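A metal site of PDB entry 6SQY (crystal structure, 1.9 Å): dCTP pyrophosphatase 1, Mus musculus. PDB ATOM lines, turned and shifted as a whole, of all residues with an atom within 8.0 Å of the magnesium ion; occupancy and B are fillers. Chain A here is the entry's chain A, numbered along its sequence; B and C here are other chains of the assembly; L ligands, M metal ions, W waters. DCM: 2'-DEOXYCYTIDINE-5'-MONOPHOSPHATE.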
ATOM      1  N   ALA A  59      10.098  13.930 -31.263  1.00  0.00           N
ATOM      2  CA  ALA A  59      10.788  15.203 -31.019  1.00  0.00           C
ATOM      3  C   ALA A  59      10.292  15.834 -29.715  1.00  0.00           C
ATOM      4  O   ALA A  59      11.103  16.388 -28.944  1.00  0.00           O
ATOM      5  CB  ALA A  59      10.618  16.140 -32.197  1.00  0.00           C
ATOM      6  N   GLY A  62      11.965  14.154 -26.821  1.00  0.00           N
ATOM      7  CA  GLY A  62      13.313  14.717 -26.715  1.00  0.00           C
ATOM      8  C   GLY A  62      13.365  16.063 -25.985  1.00  0.00           C
ATOM      9  O   GLY A  62      14.250  16.299 -25.166  1.00  0.00           O
ATOM     10  N   GLU A  63      12.400  16.922 -26.266  1.00  0.00           N
ATOM     11  CA  GLU A  63      12.358  18.255 -25.642  1.00  0.00           C
ATOM     12  C   GLU A  63      11.930  18.149 -24.181  1.00  0.00           C
ATOM     13  O   GLU A  63      12.420  18.863 -23.345  1.00  0.00           O
ATOM     14  CB  GLU A  63      11.444  19.211 -26.414  1.00  0.00           C
ATOM     15  CG  GLU A  63      11.838  19.430 -27.889  1.00  0.00           C
ATOM     16  CD  GLU A  63      13.248  19.939 -28.107  1.00  0.00           C
ATOM     17  OE1 GLU A  63      13.889  20.479 -27.160  1.00  0.00           O
ATOM     18  OE2 GLU A  63      13.727  19.815 -29.252  1.00  0.00           O
ATOM     19  N   VAL A  64      11.010  17.256 -23.890  1.00  0.00           N
ATOM     20  CA  VAL A  64      10.656  16.990 -22.487  1.00  0.00           C
ATOM     21  C   VAL A  64      11.906  16.504 -21.716  1.00  0.00           C
ATOM     22  O   VAL A  64      12.100  16.884 -20.558  1.00  0.00           O
ATOM     23  CB  VAL A  64       9.488  16.008 -22.381  1.00  0.00           C
ATOM     24  CG1 VAL A  64       9.268  15.494 -20.968  1.00  0.00           C
ATOM     25  CG2 VAL A  64       8.207  16.668 -22.869  1.00  0.00           C
ATOM     26  N   GLY A  65      12.740  15.691 -22.360  1.00  0.00           N
ATOM     27  CA  GLY A  65      14.029  15.272 -21.774  1.00  0.00           C
ATOM     28  C   GLY A  65      14.928  16.436 -21.435  1.00  0.00           C
ATOM     29  O   GLY A  65      15.475  16.496 -20.310  1.00  0.00           O
ATOM     30  N   GLU A  66      15.097  17.342 -22.394  1.00  0.00           N
ATOM     31  CA  GLU A  66      15.902  18.536 -22.164  1.00  0.00           C
ATOM     32  C   GLU A  66      15.357  19.417 -21.024  1.00  0.00           C
ATOM     33  O   GLU A  66      16.112  19.956 -20.244  1.00  0.00           O
ATOM     34  CB  GLU A  66      16.068  19.372 -23.449  1.00  0.00           C
ATOM     35  CG  GLU A  66      16.933  18.623 -24.476  1.00  0.00           C
ATOM     36  CD  GLU A  66      17.393  19.525 -25.666  1.00  0.00           C
ATOM     37  OE1 GLU A  66      18.546  19.413 -26.071  1.00  0.00           O
ATOM     38  OE2 GLU A  66      16.652  20.404 -26.129  1.00  0.00           O
ATOM     39  N   LEU A  67      14.047  19.547 -20.932  1.00  0.00           N
ATOM     40  CA  LEU A  67      13.401  20.266 -19.858  1.00  0.00           C
ATOM     41  C   LEU A  67      13.689  19.600 -18.504  1.00  0.00           C
ATOM     42  O   LEU A  67      14.102  20.260 -17.538  1.00  0.00           O
ATOM     43  CB  LEU A  67      11.895  20.336 -20.111  1.00  0.00           C
ATOM     44  CG  LEU A  67      10.989  21.048 -19.122  1.00  0.00           C
ATOM     45  CD1 LEU A  67      11.391  22.481 -19.006  1.00  0.00           C
ATOM     46  CD2 LEU A  67       9.526  20.910 -19.531  1.00  0.00           C
ATOM     47  N   ALA A  91      17.631  29.084 -20.571  1.00  0.00           N
ATOM     48  CA  ALA A  91      17.446  27.680 -20.976  1.00  0.00           C
ATOM     49  C   ALA A  91      16.029  27.192 -20.670  1.00  0.00           C
ATOM     50  O   ALA A  91      15.442  26.500 -21.485  1.00  0.00           O
ATOM     51  CB  ALA A  91      18.472  26.750 -20.359  1.00  0.00           C
ATOM     52  N   GLU A  94      13.566  28.501 -23.182  1.00  0.00           N
ATOM     53  CA  GLU A  94      13.781  27.821 -24.428  1.00  0.00           C
ATOM     54  C   GLU A  94      13.191  26.424 -24.458  1.00  0.00           C
ATOM     55  O   GLU A  94      12.499  26.086 -25.426  1.00  0.00           O
ATOM     56  CB  GLU A  94      15.249  27.769 -24.801  1.00  0.00           C
ATOM     57  CG  GLU A  94      15.774  29.177 -25.161  1.00  0.00           C
ATOM     58  CD  GLU A  94      17.265  29.190 -25.336  1.00  0.00           C
ATOM     59  OE1 GLU A  94      17.911  30.174 -24.919  1.00  0.00           O
ATOM     60  OE2 GLU A  94      17.806  28.201 -25.858  1.00  0.00           O
ATOM     61  N   GLU A  95      13.421  25.633 -23.407  1.00  0.00           N
ATOM     62  CA  GLU A  95      12.930  24.260 -23.420  1.00  0.00           C
ATOM     63  C   GLU A  95      11.419  24.170 -23.229  1.00  0.00           C
ATOM     64  O   GLU A  95      10.772  23.370 -23.930  1.00  0.00           O
ATOM     65  CB  GLU A  95      13.665  23.341 -22.426  1.00  0.00           C
ATOM     66  CG  GLU A  95      15.168  23.240 -22.605  1.00  0.00           C
ATOM     67  CD  GLU A  95      15.680  23.070 -24.044  1.00  0.00           C
ATOM     68  OE1 GLU A  95      15.016  22.442 -24.885  1.00  0.00           O
ATOM     69  OE2 GLU A  95      16.781  23.533 -24.341  1.00  0.00           O
ATOM     70  N   LEU A  96      10.842  24.992 -22.342  1.00  0.00           N
ATOM     71  CA  LEU A  96       9.385  25.106 -22.308  1.00  0.00           C
ATOM     72  C   LEU A  96       8.786  25.443 -23.677  1.00  0.00           C
ATOM     73  O   LEU A  96       7.757  24.862 -24.064  1.00  0.00           O
ATOM     74  CB  LEU A  96       8.903  26.107 -21.276  1.00  0.00           C
ATOM     75  CG  LEU A  96       9.134  25.792 -19.803  1.00  0.00           C
ATOM     76  CD1 LEU A  96       9.001  27.062 -18.992  1.00  0.00           C
ATOM     77  CD2 LEU A  96       8.213  24.705 -19.257  1.00  0.00           C
ATOM     78  N   SER A  97       9.441  26.362 -24.401  1.00  0.00           N
ATOM     79  CA  SER A  97       8.980  26.755 -25.725  1.00  0.00           C
ATOM     80  C   SER A  97       9.104  25.607 -26.724  1.00  0.00           C
ATOM     81  O   SER A  97       8.185  25.400 -27.519  1.00  0.00           O
ATOM     82  CB  SER A  97       9.761  27.982 -26.255  1.00  0.00           C
ATOM     83  OG  SER A  97       9.552  29.118 -25.414  1.00  0.00           O
ATOM     84  N   ASP A  98      10.231  24.882 -26.721  1.00  0.00           N
ATOM     85  CA  ASP A  98      10.403  23.761 -27.638  1.00  0.00           C
ATOM     86  C   ASP A  98       9.314  22.688 -27.423  1.00  0.00           C
ATOM     87  O   ASP A  98       8.804  22.134 -28.406  1.00  0.00           O
ATOM     88  CB  ASP A  98      11.764  23.072 -27.515  1.00  0.00           C
ATOM     89  CG  ASP A  98      12.913  23.834 -28.106  1.00  0.00           C
ATOM     90  OD1 ASP A  98      12.692  24.669 -28.993  1.00  0.00           O
ATOM     91  OD2 ASP A  98      14.057  23.564 -27.664  1.00  0.00           O
ATOM     92  N   VAL A  99       8.931  22.423 -26.165  1.00  0.00           N
ATOM     93  CA  VAL A  99       7.884  21.479 -25.891  1.00  0.00           C
ATOM     94  C   VAL A  99       6.535  21.986 -26.492  1.00  0.00           C
ATOM     95  O   VAL A  99       5.805  21.229 -27.128  1.00  0.00           O
ATOM     96  CB  VAL A  99       7.760  21.225 -24.381  1.00  0.00           C
ATOM     97  CG1 VAL A  99       6.536  20.359 -24.110  1.00  0.00           C
ATOM     98  CG2 VAL A  99       9.029  20.520 -23.846  1.00  0.00           C
ATOM     99  N   TYR A 102       6.414  21.754 -30.517  1.00  0.00           N
ATOM    100  CA  TYR A 102       6.103  20.417 -31.010  1.00  0.00           C
ATOM    101  C   TYR A 102       4.715  19.923 -30.639  1.00  0.00           C
ATOM    102  O   TYR A 102       4.110  19.205 -31.413  1.00  0.00           O
ATOM    103  CB  TYR A 102       7.186  19.376 -30.634  1.00  0.00           C
ATOM    104  CG  TYR A 102       8.483  19.528 -31.390  1.00  0.00           C
ATOM    105  CD1 TYR A 102       8.523  19.455 -32.774  1.00  0.00           C
ATOM    106  CD2 TYR A 102       9.685  19.747 -30.726  1.00  0.00           C
ATOM    107  CE1 TYR A 102       9.728  19.575 -33.472  1.00  0.00           C
ATOM    108  CE2 TYR A 102      10.856  19.857 -31.417  1.00  0.00           C
ATOM    109  CZ  TYR A 102      10.883  19.771 -32.785  1.00  0.00           C
ATOM    110  OH  TYR A 102      12.100  19.859 -33.441  1.00  0.00           O
ATOM    111  N   LYS B 121      12.070  31.911 -29.086  1.00  0.00           N
ATOM    112  CA  LYS B 121      12.594  30.613 -29.567  1.00  0.00           C
ATOM    113  C   LYS B 121      12.471  30.460 -31.081  1.00  0.00           C
ATOM    114  O   LYS B 121      13.401  29.982 -31.728  1.00  0.00           O
ATOM    115  CB  LYS B 121      11.959  29.406 -28.843  1.00  0.00           C
ATOM    116  CG  LYS B 121      12.734  28.096 -29.021  1.00  0.00           C
ATOM    117  CD  LYS B 121      14.205  28.220 -28.618  1.00  0.00           C
ATOM    118  CE  LYS B 121      14.979  26.918 -28.587  1.00  0.00           C
ATOM    119  NZ  LYS B 121      14.917  26.119 -29.848  1.00  0.00           N
ATOM    120  N   ASN B 125      15.294  29.785 -33.658  1.00  0.00           N
ATOM    121  CA  ASN B 125      15.192  28.678 -34.612  1.00  0.00           C
ATOM    122  C   ASN B 125      15.539  29.160 -36.056  1.00  0.00           C
ATOM    123  O   ASN B 125      16.296  28.487 -36.794  1.00  0.00           O
ATOM    124  CB  ASN B 125      13.789  28.068 -34.582  1.00  0.00           C
ATOM    125  CG  ASN B 125      13.504  27.292 -33.309  1.00  0.00           C
ATOM    126  OD1 ASN B 125      14.423  27.009 -32.541  1.00  0.00           O
ATOM    127  ND2 ASN B 125      12.216  26.983 -33.050  1.00  0.00           N
ATOM    128  N   GLU C  69      15.857  11.303 -29.403  1.00  0.00           N
ATOM    129  CA  GLU C  69      16.480  12.208 -30.373  1.00  0.00           C
ATOM    130  C   GLU C  69      17.172  11.460 -31.526  1.00  0.00           C
ATOM    131  O   GLU C  69      17.150  11.926 -32.663  1.00  0.00           O
ATOM    132  CB  GLU C  69      17.504  13.148 -29.746  1.00  0.00           C
ATOM    133  CG  GLU C  69      16.975  14.279 -28.903  1.00  0.00           C
ATOM    134  CD  GLU C  69      18.121  15.129 -28.286  1.00  0.00           C
ATOM    135  OE1 GLU C  69      19.241  15.086 -28.828  1.00  0.00           O
ATOM    136  OE2 GLU C  69      17.930  15.896 -27.271  1.00  0.00           O
HETATM  137  N1  DCM L   1      12.466  22.543 -35.526  1.00  0.00           N
HETATM  138  C2  DCM L   1      11.371  21.970 -36.250  1.00  0.00           C
HETATM  139  N3  DCM L   1      11.585  20.940 -37.126  1.00  0.00           N
HETATM  140  C4  DCM L   1      12.850  20.462 -37.342  1.00  0.00           C
HETATM  141  C5  DCM L   1      13.942  21.023 -36.656  1.00  0.00           C
HETATM  142  C6  DCM L   1      13.729  22.062 -35.752  1.00  0.00           C
HETATM  143  O2  DCM L   1      10.196  22.393 -36.032  1.00  0.00           O
HETATM  144  N4  DCM L   1      13.078  19.445 -38.202  1.00  0.00           N
HETATM  145  C1' DCM L   1      12.248  23.650 -34.559  1.00  0.00           C
HETATM  146  C2' DCM L   1      11.270  23.348 -33.406  1.00  0.00           C
HETATM  147  C3' DCM L   1      12.035  23.543 -32.078  1.00  0.00           C
HETATM  148  C4' DCM L   1      13.493  23.699 -32.488  1.00  0.00           C
HETATM  149  O4' DCM L   1      13.502  23.990 -33.918  1.00  0.00           O
HETATM  150  O3' DCM L   1      11.639  24.709 -31.319  1.00  0.00           O
HETATM  151  C5' DCM L   1      14.345  22.475 -32.182  1.00  0.00           C
HETATM  152  O5' DCM L   1      15.620  22.676 -32.785  1.00  0.00           O
HETATM  153  P   DCM L   1      16.901  21.718 -32.462  1.00  0.00           P
HETATM  154  O1P DCM L   1      17.842  22.121 -33.572  1.00  0.00           O
HETATM  155  O2P DCM L   1      17.349  22.212 -31.105  1.00  0.00           O
HETATM  156  O3P DCM L   1      16.337  20.262 -32.516  1.00  0.00           O
HETATM  157 MG    MG M   1      15.336  21.896 -26.818  1.00  0.00          MG
HETATM  158  O   HOH W   1      17.190  23.099 -26.973  1.00  0.00           O
HETATM  159  O   HOH W   2      15.977  21.357 -28.713  1.00  0.00           O
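OD1 of Asp 98 sits at hydrogen-bond distance from O3' of the ligand (2.6 Å). The side-chain amide nitrogen (ND2) of Asn 125 of chain B is in hydrogen-bond range of an oxygen (O3') of the ligand, at 2.9 Å.
OD1 of Asp 98 is in salt-bridge range of NZ of Lys 121 of chain B (2.8 Å).
The magnesium ion is bound by OE1 of Glu 95 (2.0 Å), OE1 of Glu 63 (2.1 Å), water W2 (2.1 Å), OE2 of Glu 66 (2.1 Å), water W1 (2.2 Å) and OD2 of Asp 98 (2.3 Å).
Water W2 bridges the side-chain carboxylate of Glu 63 (2.8 Å) and an oxygen (O2P) of the ligand (2.9 Å).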
